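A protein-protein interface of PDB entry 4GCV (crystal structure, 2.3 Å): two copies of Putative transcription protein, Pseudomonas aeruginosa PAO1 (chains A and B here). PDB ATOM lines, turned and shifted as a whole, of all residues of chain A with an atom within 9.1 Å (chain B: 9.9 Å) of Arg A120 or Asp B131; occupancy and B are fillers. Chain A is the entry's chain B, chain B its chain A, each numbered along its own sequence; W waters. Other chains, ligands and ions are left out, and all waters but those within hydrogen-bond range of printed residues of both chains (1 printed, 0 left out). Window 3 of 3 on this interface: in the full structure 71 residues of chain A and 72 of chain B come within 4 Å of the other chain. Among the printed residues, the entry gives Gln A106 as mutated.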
ATOM      1  N   GLN A 106      -6.672  -7.926 -21.318  1.00  0.00           N
ATOM      2  CA  GLN A 106      -8.112  -7.692 -21.374  1.00  0.00           C
ATOM      3  C   GLN A 106      -8.644  -7.316 -22.745  1.00  0.00           C
ATOM      4  O   GLN A 106      -9.565  -7.990 -23.220  1.00  0.00           O
ATOM      5  CB  GLN A 106      -8.551  -6.649 -20.360  1.00  0.00           C
ATOM      6  CG  GLN A 106      -8.696  -7.206 -18.972  1.00  0.00           C
ATOM      7  CD  GLN A 106      -7.612  -6.715 -18.022  1.00  0.00           C
ATOM      8  OE1 GLN A 106      -6.430  -6.468 -18.417  1.00  0.00           O
ATOM      9  NE2 GLN A 106      -8.004  -6.554 -16.739  1.00  0.00           N
ATOM     10  N   GLN A 112     -15.225 -12.577 -20.825  1.00  0.00           N
ATOM     11  CA  GLN A 112     -14.764 -11.889 -19.627  1.00  0.00           C
ATOM     12  C   GLN A 112     -15.683 -12.116 -18.442  1.00  0.00           C
ATOM     13  O   GLN A 112     -16.921 -12.099 -18.565  1.00  0.00           O
ATOM     14  CB  GLN A 112     -14.717 -10.395 -19.874  1.00  0.00           C
ATOM     15  CG  GLN A 112     -13.680  -9.985 -20.837  1.00  0.00           C
ATOM     16  CD  GLN A 112     -13.572  -8.492 -20.967  1.00  0.00           C
ATOM     17  OE1 GLN A 112     -14.567  -7.765 -20.840  1.00  0.00           O
ATOM     18  NE2 GLN A 112     -12.362  -8.013 -21.251  1.00  0.00           N
ATOM     19  N   LEU A 113     -15.049 -12.282 -17.286  1.00  0.00           N
ATOM     20  CA  LEU A 113     -15.721 -12.204 -16.011  1.00  0.00           C
ATOM     21  C   LEU A 113     -15.694 -10.736 -15.598  1.00  0.00           C
ATOM     22  O   LEU A 113     -14.592 -10.171 -15.431  1.00  0.00           O
ATOM     23  CB  LEU A 113     -14.975 -13.129 -15.031  1.00  0.00           C
ATOM     24  CG  LEU A 113     -15.436 -13.371 -13.595  1.00  0.00           C
ATOM     25  CD1 LEU A 113     -16.833 -14.021 -13.575  1.00  0.00           C
ATOM     26  CD2 LEU A 113     -14.399 -14.217 -12.826  1.00  0.00           C
ATOM     27  N   VAL A 114     -16.885 -10.109 -15.492  1.00  0.00           N
ATOM     28  CA  VAL A 114     -17.039  -8.709 -15.080  1.00  0.00           C
ATOM     29  C   VAL A 114     -17.996  -8.482 -13.905  1.00  0.00           C
ATOM     30  O   VAL A 114     -18.753  -9.373 -13.515  1.00  0.00           O
ATOM     31  CB  VAL A 114     -17.520  -7.771 -16.227  1.00  0.00           C
ATOM     32  CG1 VAL A 114     -16.584  -7.820 -17.436  1.00  0.00           C
ATOM     33  CG2 VAL A 114     -18.933  -8.067 -16.654  1.00  0.00           C
ATOM     34  N   GLU A 115     -17.950  -7.296 -13.331  1.00  0.00           N
ATOM     35  CA  GLU A 115     -18.940  -6.920 -12.328  1.00  0.00           C
ATOM     36  C   GLU A 115     -20.224  -6.667 -13.119  1.00  0.00           C
ATOM     37  O   GLU A 115     -20.194  -5.931 -14.087  1.00  0.00           O
ATOM     38  CB  GLU A 115     -18.548  -5.661 -11.546  1.00  0.00           C
ATOM     39  CG  GLU A 115     -19.708  -5.120 -10.671  1.00  0.00           C
ATOM     40  CD  GLU A 115     -19.378  -3.871  -9.899  1.00  0.00           C
ATOM     41  OE1 GLU A 115     -19.755  -3.784  -8.705  1.00  0.00           O
ATOM     42  OE2 GLU A 115     -18.768  -2.952 -10.474  1.00  0.00           O
ATOM     43  N   ARG A 116     -21.322  -7.321 -12.755  1.00  0.00           N
ATOM     44  CA  ARG A 116     -22.538  -7.211 -13.597  1.00  0.00           C
ATOM     45  C   ARG A 116     -23.027  -5.748 -13.752  1.00  0.00           C
ATOM     46  O   ARG A 116     -23.436  -5.349 -14.835  1.00  0.00           O
ATOM     47  CB  ARG A 116     -23.659  -8.142 -13.139  1.00  0.00           C
ATOM     48  CG  ARG A 116     -25.019  -7.909 -13.898  1.00  0.00           C
ATOM     49  CD  ARG A 116     -25.770  -9.242 -14.080  1.00  0.00           C
ATOM     50  NE  ARG A 116     -26.155  -9.488 -15.481  1.00  0.00           N
ATOM     51  CZ  ARG A 116     -26.320 -10.697 -16.027  1.00  0.00           C
ATOM     52  NH1 ARG A 116     -26.130 -11.806 -15.305  1.00  0.00           N
ATOM     53  NH2 ARG A 116     -26.671 -10.796 -17.305  1.00  0.00           N
ATOM     54  N   THR A 117     -22.924  -4.953 -12.698  1.00  0.00           N
ATOM     55  CA  THR A 117     -23.361  -3.541 -12.744  1.00  0.00           C
ATOM     56  C   THR A 117     -22.606  -2.692 -13.768  1.00  0.00           C
ATOM     57  O   THR A 117     -23.190  -2.133 -14.692  1.00  0.00           O
ATOM     58  CB  THR A 117     -23.211  -2.865 -11.363  1.00  0.00           C
ATOM     59  OG1 THR A 117     -24.332  -3.202 -10.546  1.00  0.00           O
ATOM     60  CG2 THR A 117     -23.163  -1.371 -11.510  1.00  0.00           C
ATOM     61  N   SER A 118     -21.306  -2.544 -13.571  1.00  0.00           N
ATOM     62  CA  SER A 118     -20.497  -1.722 -14.460  1.00  0.00           C
ATOM     63  C   SER A 118     -20.030  -2.718 -15.477  1.00  0.00           C
ATOM     64  O   SER A 118     -20.356  -3.903 -15.380  1.00  0.00           O
ATOM     65  CB  SER A 118     -19.312  -1.214 -13.668  1.00  0.00           C
ATOM     66  OG  SER A 118     -18.701  -2.323 -13.008  1.00  0.00           O
ATOM     67  N   GLY A 119     -19.224  -2.345 -16.443  1.00  0.00           N
ATOM     68  CA  GLY A 119     -18.667  -3.490 -17.186  1.00  0.00           C
ATOM     69  C   GLY A 119     -17.346  -3.983 -16.614  1.00  0.00           C
ATOM     70  O   GLY A 119     -16.605  -4.617 -17.315  1.00  0.00           O
ATOM     71  N   ARG A 120     -17.065  -3.698 -15.341  1.00  0.00           N
ATOM     72  CA  ARG A 120     -15.698  -3.698 -14.762  1.00  0.00           C
ATOM     73  C   ARG A 120     -15.043  -5.075 -14.679  1.00  0.00           C
ATOM     74  O   ARG A 120     -15.547  -5.968 -13.973  1.00  0.00           O
ATOM     75  CB  ARG A 120     -15.744  -3.037 -13.382  1.00  0.00           C
ATOM     76  CG  ARG A 120     -14.448  -2.404 -12.876  1.00  0.00           C
ATOM     77  CD  ARG A 120     -13.933  -1.282 -13.762  1.00  0.00           C
ATOM     78  NE  ARG A 120     -14.655  -0.016 -13.626  1.00  0.00           N
ATOM     79  CZ  ARG A 120     -15.512   0.472 -14.526  1.00  0.00           C
ATOM     80  NH1 ARG A 120     -15.776  -0.201 -15.644  1.00  0.00           N
ATOM     81  NH2 ARG A 120     -16.095   1.641 -14.309  1.00  0.00           N
ATOM     82  N   PRO A 121     -13.909  -5.272 -15.394  1.00  0.00           N
ATOM     83  CA  PRO A 121     -13.407  -6.637 -15.374  1.00  0.00           C
ATOM     84  C   PRO A 121     -12.841  -7.063 -14.019  1.00  0.00           C
ATOM     85  O   PRO A 121     -12.394  -6.246 -13.221  1.00  0.00           O
ATOM     86  CB  PRO A 121     -12.315  -6.633 -16.462  1.00  0.00           C
ATOM     87  CG  PRO A 121     -12.485  -5.368 -17.188  1.00  0.00           C
ATOM     88  CD  PRO A 121     -13.024  -4.408 -16.184  1.00  0.00           C
ATOM     89  N   VAL A 122     -12.952  -8.350 -13.771  1.00  0.00           N
ATOM     90  CA  VAL A 122     -12.426  -8.985 -12.593  1.00  0.00           C
ATOM     91  C   VAL A 122     -10.921  -9.304 -12.811  1.00  0.00           C
ATOM     92  O   VAL A 122     -10.581 -10.128 -13.678  1.00  0.00           O
ATOM     93  CB  VAL A 122     -13.178 -10.302 -12.351  1.00  0.00           C
ATOM     94  CG1 VAL A 122     -12.485 -11.145 -11.252  1.00  0.00           C
ATOM     95  CG2 VAL A 122     -14.670 -10.020 -12.031  1.00  0.00           C
ATOM     96  N   ARG A 123     -10.055  -8.665 -12.024  1.00  0.00           N
ATOM     97  CA  ARG A 123      -8.631  -9.018 -11.983  1.00  0.00           C
ATOM     98  C   ARG A 123      -8.340 -10.400 -11.411  1.00  0.00           C
ATOM     99  O   ARG A 123      -7.606 -11.154 -12.018  1.00  0.00           O
ATOM    100  CB  ARG A 123      -7.819  -7.969 -11.209  1.00  0.00           C
ATOM    101  CG  ARG A 123      -7.986  -6.547 -11.725  1.00  0.00           C
ATOM    102  CD  ARG A 123      -6.984  -5.550 -11.081  1.00  0.00           C
ATOM    103  NE  ARG A 123      -5.635  -6.117 -11.019  1.00  0.00           N
ATOM    104  CZ  ARG A 123      -5.036  -6.486  -9.893  1.00  0.00           C
ATOM    105  NH1 ARG A 123      -5.642  -6.296  -8.719  1.00  0.00           N
ATOM    106  NH2 ARG A 123      -3.820  -7.020  -9.942  1.00  0.00           N
ATOM    107  N   SER A 124      -8.899 -10.732 -10.248  1.00  0.00           N
ATOM    108  CA  SER A 124      -8.678 -12.044  -9.658  1.00  0.00           C
ATOM    109  C   SER A 124      -9.706 -12.408  -8.608  1.00  0.00           C
ATOM    110  O   SER A 124     -10.417 -11.545  -8.101  1.00  0.00           O
ATOM    111  CB  SER A 124      -7.287 -12.133  -9.018  1.00  0.00           C
ATOM    112  OG  SER A 124      -7.123 -11.085  -8.095  1.00  0.00           O
ATOM    113  N   ALA B 127     -14.408 -10.929  -5.744  1.00  0.00           N
ATOM    114  CA  ALA B 127     -13.774 -10.576  -6.965  1.00  0.00           C
ATOM    115  C   ALA B 127     -13.112  -9.229  -6.728  1.00  0.00           C
ATOM    116  O   ALA B 127     -13.806  -8.274  -6.359  1.00  0.00           O
ATOM    117  CB  ALA B 127     -14.814 -10.475  -8.075  1.00  0.00           C
ATOM    118  N   ALA B 128     -11.778  -9.182  -6.899  1.00  0.00           N
ATOM    119  CA  ALA B 128     -10.996  -7.947  -6.954  1.00  0.00           C
ATOM    120  C   ALA B 128     -11.158  -7.407  -8.357  1.00  0.00           C
ATOM    121  O   ALA B 128     -10.951  -8.142  -9.351  1.00  0.00           O
ATOM    122  CB  ALA B 128      -9.527  -8.206  -6.655  1.00  0.00           C
ATOM    123  N   LEU B 129     -11.552  -6.147  -8.453  1.00  0.00           N
ATOM    124  CA  LEU B 129     -11.847  -5.561  -9.752  1.00  0.00           C
ATOM    125  C   LEU B 129     -10.691  -4.691 -10.244  1.00  0.00           C
ATOM    126  O   LEU B 129      -9.712  -4.425  -9.493  1.00  0.00           O
ATOM    127  CB  LEU B 129     -13.172  -4.759  -9.717  1.00  0.00           C
ATOM    128  CG  LEU B 129     -14.422  -5.529  -9.260  1.00  0.00           C
ATOM    129  CD1 LEU B 129     -15.624  -4.597  -9.139  1.00  0.00           C
ATOM    130  CD2 LEU B 129     -14.809  -6.757 -10.159  1.00  0.00           C
ATOM    131  N   ALA B 130     -10.811  -4.251 -11.500  1.00  0.00           N
ATOM    132  CA  ALA B 130      -9.820  -3.355 -12.155  1.00  0.00           C
ATOM    133  C   ALA B 130      -9.681  -2.022 -11.497  1.00  0.00           C
ATOM    134  O   ALA B 130      -8.572  -1.454 -11.455  1.00  0.00           O
ATOM    135  CB  ALA B 130     -10.194  -3.133 -13.648  1.00  0.00           C
ATOM    136  N   ASP B 131     -10.804  -1.471 -11.029  1.00  0.00           N
ATOM    137  CA  ASP B 131     -10.772  -0.185 -10.302  1.00  0.00           C
ATOM    138  C   ASP B 131     -10.371  -0.251  -8.806  1.00  0.00           C
ATOM    139  O   ASP B 131     -10.569   0.716  -8.065  1.00  0.00           O
ATOM    140  CB  ASP B 131     -12.121   0.528 -10.438  1.00  0.00           C
ATOM    141  CG  ASP B 131     -13.298  -0.327  -9.948  1.00  0.00           C
ATOM    142  OD1 ASP B 131     -13.092  -1.301  -9.185  1.00  0.00           O
ATOM    143  OD2 ASP B 131     -14.440  -0.015 -10.328  1.00  0.00           O
ATOM    144  N   GLY B 132      -9.845  -1.376  -8.336  1.00  0.00           N
ATOM    145  CA  GLY B 132      -9.467  -1.469  -6.915  1.00  0.00           C
ATOM    146  C   GLY B 132     -10.543  -1.928  -5.935  1.00  0.00           C
ATOM    147  O   GLY B 132     -10.236  -2.226  -4.793  1.00  0.00           O
ATOM    148  N   ARG B 133     -11.800  -1.989  -6.371  1.00  0.00           N
ATOM    149  CA  ARG B 133     -12.886  -2.516  -5.538  1.00  0.00           C
ATOM    150  C   ARG B 133     -12.915  -4.061  -5.467  1.00  0.00           C
ATOM    151  O   ARG B 133     -12.403  -4.752  -6.348  1.00  0.00           O
ATOM    152  CB  ARG B 133     -14.242  -1.957  -6.009  1.00  0.00           C
ATOM    153  CG  ARG B 133     -14.326  -0.393  -5.978  1.00  0.00           C
ATOM    154  CD  ARG B 133     -15.720   0.144  -6.344  1.00  0.00           C
ATOM    155  NE  ARG B 133     -16.039  -0.203  -7.718  1.00  0.00           N
ATOM    156  CZ  ARG B 133     -16.965  -1.085  -8.095  1.00  0.00           C
ATOM    157  NH1 ARG B 133     -17.750  -1.689  -7.225  1.00  0.00           N
ATOM    158  NH2 ARG B 133     -17.128  -1.336  -9.376  1.00  0.00           N
ATOM    159  N   THR B 134     -13.486  -4.590  -4.386  1.00  0.00           N
ATOM    160  CA  THR B 134     -13.678  -6.007  -4.224  1.00  0.00           C
ATOM    161  C   THR B 134     -15.146  -6.245  -3.922  1.00  0.00           C
ATOM    162  O   THR B 134     -15.662  -5.705  -2.954  1.00  0.00           O
ATOM    163  CB  THR B 134     -12.837  -6.548  -3.086  1.00  0.00           C
ATOM    164  OG1 THR B 134     -11.451  -6.542  -3.455  1.00  0.00           O
ATOM    165  CG2 THR B 134     -13.217  -7.937  -2.808  1.00  0.00           C
ATOM    166  N   VAL B 135     -15.811  -7.059  -4.744  1.00  0.00           N
ATOM    167  CA  VAL B 135     -17.254  -7.263  -4.641  1.00  0.00           C
ATOM    168  C   VAL B 135     -17.527  -8.760  -4.511  1.00  0.00           C
ATOM    169  O   VAL B 135     -16.598  -9.567  -4.718  1.00  0.00           O
ATOM    170  CB  VAL B 135     -17.985  -6.747  -5.890  1.00  0.00           C
ATOM    171  CG1 VAL B 135     -17.912  -5.159  -6.015  1.00  0.00           C
ATOM    172  CG2 VAL B 135     -17.473  -7.468  -7.147  1.00  0.00           C
ATOM    173  N   PRO B 136     -18.780  -9.155  -4.146  1.00  0.00           N
ATOM    174  CA  PRO B 136     -19.048 -10.617  -4.119  1.00  0.00           C
ATOM    175  C   PRO B 136     -19.060 -11.220  -5.509  1.00  0.00           C
ATOM    176  O   PRO B 136     -19.518 -10.582  -6.474  1.00  0.00           O
ATOM    177  CB  PRO B 136     -20.416 -10.716  -3.468  1.00  0.00           C
ATOM    178  CG  PRO B 136     -20.469  -9.422  -2.576  1.00  0.00           C
ATOM    179  CD  PRO B 136     -19.861  -8.395  -3.490  1.00  0.00           C
ATOM    180  N   GLN B 139     -21.984 -11.183  -7.461  1.00  0.00           N
ATOM    181  CA  GLN B 139     -22.334  -9.974  -8.230  1.00  0.00           C
ATOM    182  C   GLN B 139     -21.580  -9.825  -9.573  1.00  0.00           C
ATOM    183  O   GLN B 139     -21.680  -8.805 -10.272  1.00  0.00           O
ATOM    184  CB  GLN B 139     -22.127  -8.730  -7.363  1.00  0.00           C
ATOM    185  CG  GLN B 139     -22.699  -8.836  -5.928  1.00  0.00           C
ATOM    186  CD  GLN B 139     -22.585  -7.534  -5.135  1.00  0.00           C
ATOM    187  OE1 GLN B 139     -23.084  -7.437  -4.004  1.00  0.00           O
ATOM    188  NE2 GLN B 139     -21.932  -6.526  -5.719  1.00  0.00           N
ATOM    189  N   CYS B 140     -20.803 -10.823  -9.933  1.00  0.00           N
ATOM    190  CA  CYS B 140     -20.127 -10.784 -11.230  1.00  0.00           C
ATOM    191  C   CYS B 140     -20.862 -11.627 -12.273  1.00  0.00           C
ATOM    192  O   CYS B 140     -21.769 -12.406 -11.935  1.00  0.00           O
ATOM    193  CB  CYS B 140     -18.671 -11.228 -11.094  1.00  0.00           C
ATOM    194  SG  CYS B 140     -17.841 -10.192  -9.872  1.00  0.00           S
ATOM    195  N   THR B 141     -20.472 -11.491 -13.534  1.00  0.00           N
ATOM    196  CA  THR B 141     -21.069 -12.353 -14.559  1.00  0.00           C
ATOM    197  C   THR B 141     -20.087 -12.614 -15.695  1.00  0.00           C
ATOM    198  O   THR B 141     -19.158 -11.835 -15.909  1.00  0.00           O
ATOM    199  CB  THR B 141     -22.396 -11.712 -15.095  1.00  0.00           C
ATOM    200  OG1 THR B 141     -22.958 -12.526 -16.136  1.00  0.00           O
ATOM    201  CG2 THR B 141     -22.134 -10.323 -15.644  1.00  0.00           C
ATOM    202  N   VAL B 142     -20.289 -13.719 -16.410  1.00  0.00           N
ATOM    203  CA  VAL B 142     -19.533 -13.992 -17.645  1.00  0.00           C
ATOM    204  C   VAL B 142     -20.213 -13.284 -18.795  1.00  0.00           C
ATOM    205  O   VAL B 142     -21.411 -13.478 -18.989  1.00  0.00           O
ATOM    206  CB  VAL B 142     -19.430 -15.515 -17.934  1.00  0.00           C
ATOM    207  CG1 VAL B 142     -18.722 -15.756 -19.265  1.00  0.00           C
ATOM    208  CG2 VAL B 142     -18.667 -16.191 -16.806  1.00  0.00           C
ATOM    209  N   GLN B 143     -19.472 -12.443 -19.526  1.00  0.00           N
ATOM    210  CA  GLN B 143     -19.998 -11.740 -20.710  1.00  0.00           C
ATOM    211  C   GLN B 143     -18.992 -11.638 -21.875  1.00  0.00           C
ATOM    212  O   GLN B 143     -17.784 -11.930 -21.712  1.00  0.00           O
ATOM    213  CB  GLN B 143     -20.525 -10.350 -20.341  1.00  0.00           C
ATOM    214  CG  GLN B 143     -19.488  -9.260 -20.290  1.00  0.00           C
ATOM    215  CD  GLN B 143     -20.106  -7.843 -20.149  1.00  0.00           C
ATOM    216  OE1 GLN B 143     -21.313  -7.708 -20.001  1.00  0.00           O
ATOM    217  NE2 GLN B 143     -19.261  -6.795 -20.205  1.00  0.00           N
ATOM    218  N   ALA B 144     -19.485 -11.250 -23.056  1.00  0.00           N
ATOM    219  CA  ALA B 144     -18.625 -11.113 -24.228  1.00  0.00           C
ATOM    220  C   ALA B 144     -17.540 -10.062 -24.017  1.00  0.00           C
ATOM    221  O   ALA B 144     -17.806  -8.966 -23.543  1.00  0.00           O
ATOM    222  CB  ALA B 144     -19.444 -10.780 -25.464  1.00  0.00           C
HETATM  223  O   HOH W   1     -22.788  -6.467  -9.649  1.00  0.00           O
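The backbone carbonyl oxygen (O) of Ala B128 is in hydrogen-bond range of the backbone NH (N) of Arg A123, 2.9 Å away.
O of Ser A124 sits at hydrogen-bond distance from N of Ala B128, at 3.0 Å.
The backbone carbonyl oxygen (O) of Pro A121 lies within hydrogen-bond range of the backbone NH (N) of Ala B130, 3.1 Å away.
The side-chain carboxylate (OD2) of Asp B131 lies within salt-bridge range of the guanidinium group (NE) of Arg A120 (3.3 Å).
NH2 of Arg B133 lies within salt-bridge range of OE2 of Glu A115.
The backbone carbonyl oxygen (O) of Gln B139 sits at hydrogen-bond distance from the backbone NH (N) of Arg A116.
O of Val A114 lies within hydrogen-bond range of N of Thr B141.
NH1 of Arg A116 sits at hydrogen-bond distance from OG1 of Thr B141 (3.4 Å).
The backbone NH (N) of Gln B143 sits at hydrogen-bond distance from the backbone carbonyl oxygen (O) of Gln A112, 2.7 Å away.
The backbone carbonyl oxygen (O) of Gln A112 lies close to the backbone carbonyl oxygen (O) of Thr B141, 3.5 Å away.
N of Ala B127 is in hydrogen-bond range of O of Val B135, at 2.8 Å.
The guanidinium group of Arg B133 is in salt-bridge range of the side-chain carboxylate of Asp B131 (3.1 Å).
The backbone carbonyl oxygen of Gln A106 is in hydrogen-bond range of the side-chain amide nitrogen of Gln A112, 3.4 Å away.
The backbone NH (N) of Val A122 sits at hydrogen-bond distance from the backbone carbonyl oxygen (O) of Leu A113.
OG of Ser A118 is in hydrogen-bond range of OE2 of Glu A115 (2.6 Å).
The side-chain hydroxyl (OG) of Ser A118 lies close to the backbone NH (N) of Arg A120, at 3.2 Å.
Arg A120 touches just these residues of chain B: Leu B129 and Asp B131.
Printed residues of chain A within 4 Å of Asp B131: Arg A120.
Of chain B, only Cys B140 (3.0 Å), Thr B141 (2.7 Å) and Gln B143 (3.7 Å) come within 4 Å of Val A114.
No residue of chain B comes within 4 Å of Ser A118.
No residue of chain B comes within 4 Å of Gly A119.
Of chain A, only Pro A121 (3.1 Å) and Arg A123 (3.6 Å) come within 4 Å of Ala B130.
Of the printed residues of chain A, Cys B140 touches Val A114, Arg A116 and Val A122.
Printed residues of chain B within 4 Å of Val A122: Ala B127 (3.98 Å), Ala B128 (3.7 Å), Leu B129 (3.8 Å) and Cys B140 (3.8 Å).
Of the printed residues of chain B, Arg A123 touches Ala B128, Leu B129 and Ala B130.
Gln A106 touches none of the printed residues of chain B.
Pro B136 touches none of the printed residues of chain A.
The nearest residue of chain B that does not touch Arg A120 is Ala B130 (4.2 Å).
The nearest residue of chain A that does not touch Asp B131 is Glu A115 (5.2 Å).
No position is printed for both chains.
Of the 27 pairs that touch across the chains among the printed residues, none has its exchanged pair printed and touching as well.
Water W1 lies within hydrogen-bond range of O of Gln B139 (2.7 Å) and N of Thr A117 (3.4 Å).
Val B142 touches Gln A112.
CA of Leu A113 touches O of Thr B141, at 3.5 Å.
Val A114 touches Cys B140.
CG2 of Val A114 touches CD of Gln B143, at 3.7 Å.
OE2 of Glu A115 touches CD1 of Leu B129, at 3.8 Å.
Arg A116 touches Cys B140 (N to CA, 3.97 Å).
Val A122 touches Ala B128 (C to O, 3.7 Å).
Cys B140 touches Val A122.
Arg A123 touches Ala B130 (CG to N, 3.6 Å).
Ser A124 touches Ala B127.
Printed residues of chain A that touch a printed residue of chain B: Gln A112, Leu A113, Val A114, Glu A115, Arg A116, Arg A120, Pro A121, Val A122, Arg A123 and Ser A124.
Hydrophobic or aromatic side chains of chain A within 4 Å of the printed part of chain B: Leu A113, Val A114 and Val A122.
Among the printed residues, 27 pairs touch across the chains.
Among the printed residues, Asp or Glu carboxylates within 4 Å of a Lys or Arg side-chain nitrogen of the other chain: Glu A115 with Arg B133 (2.6 Å) and Arg A120 with Asp B131 (3.3 Å).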
